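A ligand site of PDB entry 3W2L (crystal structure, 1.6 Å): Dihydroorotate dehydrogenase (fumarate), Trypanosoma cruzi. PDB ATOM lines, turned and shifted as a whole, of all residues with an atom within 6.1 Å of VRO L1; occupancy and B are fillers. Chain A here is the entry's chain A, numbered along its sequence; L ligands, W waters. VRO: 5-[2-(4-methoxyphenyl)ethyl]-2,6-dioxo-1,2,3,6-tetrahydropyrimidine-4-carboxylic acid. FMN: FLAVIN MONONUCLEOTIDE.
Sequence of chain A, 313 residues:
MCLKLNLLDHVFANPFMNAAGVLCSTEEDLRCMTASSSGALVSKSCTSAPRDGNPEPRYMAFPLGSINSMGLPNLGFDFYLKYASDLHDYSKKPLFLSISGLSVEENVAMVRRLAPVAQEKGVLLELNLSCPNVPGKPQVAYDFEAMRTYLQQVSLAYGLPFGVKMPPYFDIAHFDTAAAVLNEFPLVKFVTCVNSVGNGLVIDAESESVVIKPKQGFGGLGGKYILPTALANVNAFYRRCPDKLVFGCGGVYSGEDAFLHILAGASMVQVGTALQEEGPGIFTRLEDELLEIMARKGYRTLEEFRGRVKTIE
Water W3 lies within hydrogen-bond range of OAN of VRO L1, N of Gly 71 and ND2 of Asn 54.
Water W1 lies within hydrogen-bond range of OAE of VRO L1 (2.8 Å) and OD1 of Asn 68 (3.1 Å).
Water W2 bridges OAN of VRO L1 (2.8 Å) and ND2 of Asn 54 (3.1 Å).
An oxygen (OAE) of VRO L1 lies within hydrogen-bond range of the backbone NH (N) of Gly 71, 3.1 Å away.
The side-chain amide nitrogen of Asn 195 is in hydrogen-bond range of an oxygen (O2) of FMN L2, at 3.5 Å.
The side-chain hydroxyl of Ser 45 lies within hydrogen-bond range of a nitrogen (N3) of FMN L2, 2.8 Å away.
The side-chain amide nitrogen (ND2) of Asn 128 is in hydrogen-bond range of an oxygen (O2) of FMN L2.
NZ of Lys 44 is in hydrogen-bond range of O4 of FMN L2 (2.7 Å).
N of Met 70 lies within hydrogen-bond range of OAE of VRO L1 (3.2 Å).
OG of Ser 196 is in hydrogen-bond range of OAC of VRO L1, at 2.9 Å.
An oxygen (O2') of FMN L2 is in hydrogen-bond range of the backbone NH of Ala 20 (3.5 Å).
The side-chain amide oxygen (OD1) of Asn 195 is in hydrogen-bond range of a nitrogen (NAM) of VRO L1, at 2.9 Å.
The side-chain amide nitrogen of Asn 128 is in hydrogen-bond range of an oxygen (OAD) of VRO L1, 3.0 Å away.
The side-chain amino group (NZ) of Lys 44 is in salt-bridge range of an oxygen (OAB) of VRO L1 (3.0 Å).
O2' of FMN L2 lies within hydrogen-bond range of O of Ala 20 (2.8 Å).
The side-chain amino group (NZ) of Lys 165 lies within hydrogen-bond range of an oxygen (O2') of FMN L2 (2.8 Å).
ND2 of Asn 68 lies within hydrogen-bond range of OAC of VRO L1, at 2.9 Å.
The backbone NH (N) of Leu 72 is in hydrogen-bond range of an oxygen (OAB) of VRO L1 (2.8 Å).
Residues that only touch VRO L1: Ser 130 (3.7 Å), Pro 132 (3.7 Å) and Lys 215 (3.6 Å).
ND2 of Asn 195 is in hydrogen-bond range of OD1 of Asn 128, at 3.4 Å.
OG of Ser 130 lies within hydrogen-bond range of ND2 of Asn 195, at 3.2 Å.
The side-chain amide oxygen (OD1) of Asn 128 lies within hydrogen-bond range of the backbone NH (N) of Ser 130 (3.0 Å).
N of Asn 54 sits at hydrogen-bond distance from O of Met 70, 2.8 Å away.
The side-chain hydroxyl of Ser 130 is in hydrogen-bond range of the backbone carbonyl oxygen of Lys 165 (2.9 Å).
The backbone carbonyl oxygen of Gly 71 sits at hydrogen-bond distance from the guanidinium group of Arg 51 (2.9 Å).
The side-chain amide oxygen (OD1) of Asn 68 is in hydrogen-bond range of the backbone NH (N) of Met 70, 3.3 Å away.
OD1 of Asn 195 is in hydrogen-bond range of OG of Ser 196 (3.5 Å).
A nitrogen (NAM) of VRO L1 sits close to a nitrogen (N1) of FMN L2 (3.5 Å).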
ATOM      1  N   ALA A  20      34.724  21.133  -6.782  1.00  0.00           N
ATOM      2  CA  ALA A  20      33.314  21.261  -6.572  1.00  0.00           C
ATOM      3  C   ALA A  20      32.601  20.286  -7.480  1.00  0.00           C
ATOM      4  O   ALA A  20      32.993  20.059  -8.598  1.00  0.00           O
ATOM      5  CB  ALA A  20      32.851  22.711  -6.749  1.00  0.00           C
ATOM      6  N   LYS A  44      29.069  21.225  -3.227  1.00  0.00           N
ATOM      7  CA  LYS A  44      28.452  21.223  -4.539  1.00  0.00           C
ATOM      8  C   LYS A  44      27.883  22.614  -4.885  1.00  0.00           C
ATOM      9  O   LYS A  44      27.195  23.190  -4.118  1.00  0.00           O
ATOM     10  CB  LYS A  44      27.323  20.187  -4.610  1.00  0.00           C
ATOM     11  CG  LYS A  44      26.515  20.178  -5.866  1.00  0.00           C
ATOM     12  CD  LYS A  44      27.257  19.836  -7.148  1.00  0.00           C
ATOM     13  CE  LYS A  44      26.457  20.173  -8.440  1.00  0.00           C
ATOM     14  NZ  LYS A  44      27.205  19.786  -9.773  1.00  0.00           N
ATOM     15  N   SER A  45      28.212  23.076  -6.074  1.00  0.00           N
ATOM     16  CA  SER A  45      27.635  24.335  -6.610  1.00  0.00           C
ATOM     17  C   SER A  45      26.138  24.262  -6.454  1.00  0.00           C
ATOM     18  O   SER A  45      25.531  23.304  -6.822  1.00  0.00           O
ATOM     19  CB  SER A  45      27.959  24.633  -8.035  1.00  0.00           C
ATOM     20  OG  SER A  45      29.333  24.912  -8.226  1.00  0.00           O
ATOM     21  N   ARG A  51      17.625  21.026  -7.119  1.00  0.00           N
ATOM     22  CA  ARG A  51      17.520  20.518  -8.466  1.00  0.00           C
ATOM     23  C   ARG A  51      17.855  19.035  -8.540  1.00  0.00           C
ATOM     24  O   ARG A  51      18.758  18.580  -7.896  1.00  0.00           O
ATOM     25  CB  ARG A  51      18.540  21.185  -9.329  1.00  0.00           C
ATOM     26  CG  ARG A  51      18.203  22.615  -9.633  1.00  0.00           C
ATOM     27  CD  ARG A  51      19.320  23.278 -10.378  1.00  0.00           C
ATOM     28  NE  ARG A  51      19.624  22.676 -11.648  1.00  0.00           N
ATOM     29  CZ  ARG A  51      19.030  22.982 -12.775  1.00  0.00           C
ATOM     30  NH1 ARG A  51      18.077  23.906 -12.778  1.00  0.00           N
ATOM     31  NH2 ARG A  51      19.372  22.353 -13.867  1.00  0.00           N
ATOM     32  N   ASN A  54      20.120  16.565 -14.552  1.00  0.00           N
ATOM     33  CA  ASN A  54      19.809  15.923 -15.824  1.00  0.00           C
ATOM     34  C   ASN A  54      19.583  14.418 -15.755  1.00  0.00           C
ATOM     35  O   ASN A  54      19.983  13.793 -14.849  1.00  0.00           O
ATOM     36  CB  ASN A  54      20.935  16.174 -16.821  1.00  0.00           C
ATOM     37  CG  ASN A  54      20.976  17.587 -17.357  1.00  0.00           C
ATOM     38  OD1 ASN A  54      20.019  18.303 -17.278  1.00  0.00           O
ATOM     39  ND2 ASN A  54      22.118  17.995 -17.854  1.00  0.00           N
ATOM     40  N   ASN A  68      30.916  14.706 -18.224  1.00  0.00           N
ATOM     41  CA  ASN A  68      29.699  14.917 -17.424  1.00  0.00           C
ATOM     42  C   ASN A  68      28.811  15.991 -17.935  1.00  0.00           C
ATOM     43  O   ASN A  68      29.251  17.012 -18.430  1.00  0.00           O
ATOM     44  CB  ASN A  68      30.001  15.166 -15.943  1.00  0.00           C
ATOM     45  CG  ASN A  68      30.189  16.645 -15.603  1.00  0.00           C
ATOM     46  OD1 ASN A  68      29.230  17.435 -15.409  1.00  0.00           O
ATOM     47  ND2 ASN A  68      31.454  17.072 -15.544  1.00  0.00           N
ATOM     48  N   SER A  69      27.513  15.743 -17.810  1.00  0.00           N
ATOM     49  CA  SER A  69      26.518  16.793 -17.995  1.00  0.00           C
ATOM     50  C   SER A  69      25.565  16.603 -16.858  1.00  0.00           C
ATOM     51  O   SER A  69      24.434  16.219 -17.081  1.00  0.00           O
ATOM     52  CB  SER A  69      25.810  16.744 -19.373  1.00  0.00           C
ATOM     53  OG  SER A  69      26.752  17.108 -20.386  1.00  0.00           O
ATOM     54  N   MET A  70      26.009  16.872 -15.646  1.00  0.00           N
ATOM     55  CA  MET A  70      25.156  16.635 -14.475  1.00  0.00           C
ATOM     56  C   MET A  70      23.884  17.482 -14.459  1.00  0.00           C
ATOM     57  O   MET A  70      22.827  17.040 -13.983  1.00  0.00           O
ATOM     58  CB  MET A  70      25.963  16.891 -13.226  1.00  0.00           C
ATOM     59  CG  MET A  70      27.232  16.079 -13.055  1.00  0.00           C
ATOM     60  SD  MET A  70      27.063  14.328 -13.117  1.00  0.00           S
ATOM     61  CE  MET A  70      26.338  14.037 -11.551  1.00  0.00           C
ATOM     62  N   GLY A  71      23.965  18.724 -14.940  1.00  0.00           N
ATOM     63  CA  GLY A  71      22.825  19.675 -14.846  1.00  0.00           C
ATOM     64  C   GLY A  71      22.620  20.308 -13.505  1.00  0.00           C
ATOM     65  O   GLY A  71      21.491  20.556 -13.120  1.00  0.00           O
ATOM     66  N   LEU A  72      23.662  20.469 -12.705  1.00  0.00           N
ATOM     67  CA  LEU A  72      23.584  21.062 -11.395  1.00  0.00           C
ATOM     68  C   LEU A  72      22.598  20.428 -10.422  1.00  0.00           C
ATOM     69  O   LEU A  72      21.826  21.116  -9.730  1.00  0.00           O
ATOM     70  CB  LEU A  72      23.320  22.553 -11.554  1.00  0.00           C
ATOM     71  CG  LEU A  72      23.884  23.595 -10.641  1.00  0.00           C
ATOM     72  CD1 LEU A  72      25.324  23.503 -10.231  1.00  0.00           C
ATOM     73  CD2 LEU A  72      23.628  24.927 -11.439  1.00  0.00           C
ATOM     74  N   PRO A  73      22.630  19.135 -10.263  1.00  0.00           N
ATOM     75  CA  PRO A  73      21.834  18.526  -9.141  1.00  0.00           C
ATOM     76  C   PRO A  73      22.394  18.946  -7.820  1.00  0.00           C
ATOM     77  O   PRO A  73      23.608  18.976  -7.627  1.00  0.00           O
ATOM     78  CB  PRO A  73      22.028  17.015  -9.331  1.00  0.00           C
ATOM     79  CG  PRO A  73      23.336  16.883 -10.032  1.00  0.00           C
ATOM     80  CD  PRO A  73      23.635  18.178 -10.793  1.00  0.00           C
ATOM     81  N   SER A 100      26.254  28.612  -7.791  1.00  0.00           N
ATOM     82  CA  SER A 100      26.100  28.701  -9.200  1.00  0.00           C
ATOM     83  C   SER A 100      24.680  29.051  -9.615  1.00  0.00           C
ATOM     84  O   SER A 100      24.053  28.320 -10.299  1.00  0.00           O
ATOM     85  CB  SER A 100      26.532  27.356  -9.797  1.00  0.00           C
ATOM     86  OG  SER A 100      26.316  27.335 -11.125  1.00  0.00           O
ATOM     87  N   LEU A 102      21.601  30.696 -11.587  1.00  0.00           N
ATOM     88  CA  LEU A 102      21.261  30.655 -12.983  1.00  0.00           C
ATOM     89  C   LEU A 102      21.009  32.057 -13.599  1.00  0.00           C
ATOM     90  O   LEU A 102      20.787  32.212 -14.760  1.00  0.00           O
ATOM     91  CB  LEU A 102      20.061  29.777 -13.196  1.00  0.00           C
ATOM     92  CG  LEU A 102      20.285  28.323 -12.773  1.00  0.00           C
ATOM     93  CD1 LEU A 102      19.106  27.460 -13.142  1.00  0.00           C
ATOM     94  CD2 LEU A 102      21.534  27.738 -13.272  1.00  0.00           C
ATOM     95  N   ASN A 128      30.908  30.180  -9.050  1.00  0.00           N
ATOM     96  CA  ASN A 128      31.141  29.490 -10.266  1.00  0.00           C
ATOM     97  C   ASN A 128      30.670  30.290 -11.463  1.00  0.00           C
ATOM     98  O   ASN A 128      29.528  30.462 -11.666  1.00  0.00           O
ATOM     99  CB  ASN A 128      30.351  28.190 -10.219  1.00  0.00           C
ATOM    100  CG  ASN A 128      30.574  27.284 -11.426  1.00  0.00           C
ATOM    101  OD1 ASN A 128      31.314  27.531 -12.259  1.00  0.00           O
ATOM    102  ND2 ASN A 128      29.872  26.214 -11.437  1.00  0.00           N
ATOM    103  N   SER A 130      31.510  29.452 -14.552  1.00  0.00           N
ATOM    104  CA  SER A 130      31.670  28.558 -15.680  1.00  0.00           C
ATOM    105  C   SER A 130      30.371  27.904 -15.719  1.00  0.00           C
ATOM    106  O   SER A 130      30.260  26.768 -15.437  1.00  0.00           O
ATOM    107  CB  SER A 130      32.836  27.549 -15.515  1.00  0.00           C
ATOM    108  OG  SER A 130      33.820  27.939 -14.466  1.00  0.00           O
ATOM    109  N   CYS A 131      29.373  28.675 -16.016  1.00  0.00           N
ATOM    110  CA  CYS A 131      28.057  28.366 -15.741  1.00  0.00           C
ATOM    111  C   CYS A 131      27.013  29.092 -16.705  1.00  0.00           C
ATOM    112  O   CYS A 131      27.125  30.198 -17.064  1.00  0.00           O
ATOM    113  CB  CYS A 131      27.872  29.008 -14.398  1.00  0.00           C
ATOM    114  SG  CYS A 131      26.219  28.979 -13.782  1.00  0.00           S
ATOM    115  N   PRO A 132      25.845  28.346 -16.945  1.00  0.00           N
ATOM    116  CA  PRO A 132      24.820  28.991 -17.773  1.00  0.00           C
ATOM    117  C   PRO A 132      24.267  30.346 -17.400  1.00  0.00           C
ATOM    118  O   PRO A 132      23.966  30.609 -16.310  1.00  0.00           O
ATOM    119  CB  PRO A 132      23.637  28.052 -17.590  1.00  0.00           C
ATOM    120  CG  PRO A 132      24.219  26.741 -17.577  1.00  0.00           C
ATOM    121  CD  PRO A 132      25.364  26.882 -16.688  1.00  0.00           C
ATOM    122  N   LYS A 165      35.487  30.407  -9.737  1.00  0.00           N
ATOM    123  CA  LYS A 165      35.848  29.199 -10.467  1.00  0.00           C
ATOM    124  C   LYS A 165      35.675  29.521 -11.995  1.00  0.00           C
ATOM    125  O   LYS A 165      34.585  29.952 -12.478  1.00  0.00           O
ATOM    126  CB  LYS A 165      34.875  28.080 -10.129  1.00  0.00           C
ATOM    127  CG  LYS A 165      35.110  26.786 -10.880  1.00  0.00           C
ATOM    128  CD  LYS A 165      36.310  26.013 -10.428  1.00  0.00           C
ATOM    129  CE  LYS A 165      36.336  24.604 -10.931  1.00  0.00           C
ATOM    130  NZ  LYS A 165      35.417  23.701 -10.249  1.00  0.00           N
ATOM    131  N   ASN A 195      37.557  24.812 -14.442  1.00  0.00           N
ATOM    132  CA  ASN A 195      36.405  23.917 -14.584  1.00  0.00           C
ATOM    133  C   ASN A 195      36.616  22.967 -15.804  1.00  0.00           C
ATOM    134  O   ASN A 195      37.605  23.024 -16.423  1.00  0.00           O
ATOM    135  CB  ASN A 195      35.164  24.796 -14.767  1.00  0.00           C
ATOM    136  CG  ASN A 195      33.901  24.171 -14.229  1.00  0.00           C
ATOM    137  OD1 ASN A 195      33.665  23.084 -14.452  1.00  0.00           O
ATOM    138  ND2 ASN A 195      33.132  24.937 -13.546  1.00  0.00           N
ATOM    139  N   SER A 196      35.638  22.117 -16.090  1.00  0.00           N
ATOM    140  CA  SER A 196      35.835  21.142 -17.119  1.00  0.00           C
ATOM    141  C   SER A 196      36.039  21.770 -18.493  1.00  0.00           C
ATOM    142  O   SER A 196      35.634  22.864 -18.703  1.00  0.00           O
ATOM    143  CB  SER A 196      34.616  20.189 -17.142  1.00  0.00           C
ATOM    144  OG  SER A 196      33.474  20.856 -17.137  1.00  0.00           O
ATOM    145  N   LYS A 215      22.157  16.287 -23.718  1.00  0.00           N
ATOM    146  CA  LYS A 215      22.861  17.112 -24.709  1.00  0.00           C
ATOM    147  C   LYS A 215      23.497  16.280 -25.849  1.00  0.00           C
ATOM    148  O   LYS A 215      24.551  16.579 -26.348  1.00  0.00           O
ATOM    149  CB  LYS A 215      23.917  18.013 -24.055  1.00  0.00           C
ATOM    150  CG  LYS A 215      23.372  18.948 -22.991  1.00  0.00           C
ATOM    151  CD  LYS A 215      24.494  19.785 -22.398  1.00  0.00           C
ATOM    152  CE  LYS A 215      25.618  20.237 -23.362  1.00  0.00           C
ATOM    153  NZ  LYS A 215      26.505  21.249 -22.715  1.00  0.00           N
ATOM    154  N   GLY A 220      31.176  18.136 -20.231  1.00  0.00           N
ATOM    155  CA  GLY A 220      32.462  18.635 -19.841  1.00  0.00           C
ATOM    156  C   GLY A 220      33.474  17.557 -19.529  1.00  0.00           C
ATOM    157  O   GLY A 220      33.154  16.561 -18.889  1.00  0.00           O
ATOM    158  N   LEU A 221      34.733  17.799 -19.917  1.00  0.00           N
ATOM    159  CA  LEU A 221      35.811  16.789 -19.772  1.00  0.00           C
ATOM    160  C   LEU A 221      36.690  17.110 -18.623  1.00  0.00           C
ATOM    161  O   LEU A 221      37.005  18.297 -18.372  1.00  0.00           O
ATOM    162  CB  LEU A 221      36.668  16.834 -20.991  1.00  0.00           C
ATOM    163  CG  LEU A 221      36.016  16.554 -22.352  1.00  0.00           C
ATOM    164  CD1 LEU A 221      37.041  16.845 -23.448  1.00  0.00           C
ATOM    165  CD2 LEU A 221      35.496  15.176 -22.439  1.00  0.00           C
HETATM  166  OAB VRO L   1      26.479  20.282 -12.664  1.00  0.00           O
HETATM  167  CAO VRO L   1      27.212  20.277 -13.675  1.00  0.00           C
HETATM  168  OAE VRO L   1      26.847  19.783 -14.756  1.00  0.00           O
HETATM  169  CAR VRO L   1      28.573  20.930 -13.708  1.00  0.00           C
HETATM  170  NAL VRO L   1      29.570  20.112 -14.301  1.00  0.00           N
HETATM  171  CAT VRO L   1      30.862  20.583 -14.521  1.00  0.00           C
HETATM  172  OAC VRO L   1      31.744  19.901 -15.079  1.00  0.00           O
HETATM  173  NAM VRO L   1      31.080  21.869 -14.060  1.00  0.00           N
HETATM  174  CAU VRO L   1      30.116  22.738 -13.507  1.00  0.00           C
HETATM  175  OAD VRO L   1      30.443  23.875 -13.163  1.00  0.00           O
HETATM  176  CAS VRO L   1      28.802  22.241 -13.392  1.00  0.00           C
HETATM  177  CAK VRO L   1      27.798  23.069 -12.834  1.00  0.00           C
HETATM  178  CAJ VRO L   1      27.399  24.286 -13.770  1.00  0.00           C
HETATM  179  CAP VRO L   1      26.727  23.770 -14.868  1.00  0.00           C
HETATM  180  CAF VRO L   1      25.385  23.662 -14.862  1.00  0.00           C
HETATM  181  CAH VRO L   1      24.617  23.132 -15.928  1.00  0.00           C
HETATM  182  CAQ VRO L   1      25.284  22.628 -17.037  1.00  0.00           C
HETATM  183  OAN VRO L   1      24.543  22.101 -18.090  1.00  0.00           O
HETATM  184  CAA VRO L   1      25.190  22.032 -19.417  1.00  0.00           C
HETATM  185  CAI VRO L   1      26.703  22.706 -17.075  1.00  0.00           C
HETATM  186  CAG VRO L   1      27.420  23.275 -15.988  1.00  0.00           C
HETATM  187  N1  FMN L   2      32.648  22.421 -11.010  1.00  0.00           N
HETATM  188  C2  FMN L   2      31.960  23.359 -10.339  1.00  0.00           C
HETATM  189  O2  FMN L   2      32.574  24.445 -10.144  1.00  0.00           O
HETATM  190  N3  FMN L   2      30.783  23.133  -9.770  1.00  0.00           N
HETATM  191  C4  FMN L   2      30.157  21.916  -9.834  1.00  0.00           C
HETATM  192  O4  FMN L   2      29.015  21.703  -9.278  1.00  0.00           O
HETATM  193  C4A FMN L   2      30.805  20.887 -10.569  1.00  0.00           C
HETATM  194  N5  FMN L   2      30.194  19.698 -10.682  1.00  0.00           N
HETATM  195  C5A FMN L   2      30.931  18.657 -11.271  1.00  0.00           C
HETATM  196  C6  FMN L   2      30.419  17.342 -11.174  1.00  0.00           C
HETATM  197  C7  FMN L   2      31.125  16.280 -11.746  1.00  0.00           C
HETATM  198  C7M FMN L   2      30.534  14.900 -11.757  1.00  0.00           C
HETATM  199  C8  FMN L   2      32.451  16.523 -12.298  1.00  0.00           C
HETATM  200  C8M FMN L   2      33.257  15.396 -12.906  1.00  0.00           C
HETATM  201  C9  FMN L   2      32.981  17.809 -12.322  1.00  0.00           C
HETATM  202  C9A FMN L   2      32.264  18.890 -11.787  1.00  0.00           C
HETATM  203  N10 FMN L   2      32.741  20.216 -11.823  1.00  0.00           N
HETATM  204  C10 FMN L   2      32.103  21.213 -11.145  1.00  0.00           C
HETATM  205  C1' FMN L   2      34.081  20.513 -12.323  1.00  0.00           C
HETATM  206  C2' FMN L   2      35.186  20.099 -11.407  1.00  0.00           C
HETATM  207  O2' FMN L   2      35.070  20.887 -10.239  1.00  0.00           O
HETATM  208  C3' FMN L   2      36.534  20.252 -12.040  1.00  0.00           C
HETATM  209  O3' FMN L   2      36.688  21.651 -12.347  1.00  0.00           O
HETATM  210  C4' FMN L   2      36.715  19.427 -13.334  1.00  0.00           C
HETATM  211  O4' FMN L   2      36.187  18.086 -13.134  1.00  0.00           O
HETATM  212  C5' FMN L   2      38.227  19.268 -13.627  1.00  0.00           C
HETATM  213  O5' FMN L   2      39.016  18.685 -12.657  1.00  0.00           O
HETATM  214  P   FMN L   2      39.494  17.153 -12.785  1.00  0.00           P
HETATM  215  O1P FMN L   2      40.183  16.809 -11.493  1.00  0.00           O
HETATM  216  O2P FMN L   2      40.325  17.041 -14.037  1.00  0.00           O
HETATM  217  O3P FMN L   2      38.184  16.332 -12.967  1.00  0.00           O
HETATM  218  O   HOH W   1      28.389  19.870 -17.113  1.00  0.00           O
HETATM  219  O   HOH W   2      22.245  20.794 -19.115  1.00  0.00           O
HETATM  220  O   HOH W   3      24.928  19.736 -17.715  1.00  0.00           O
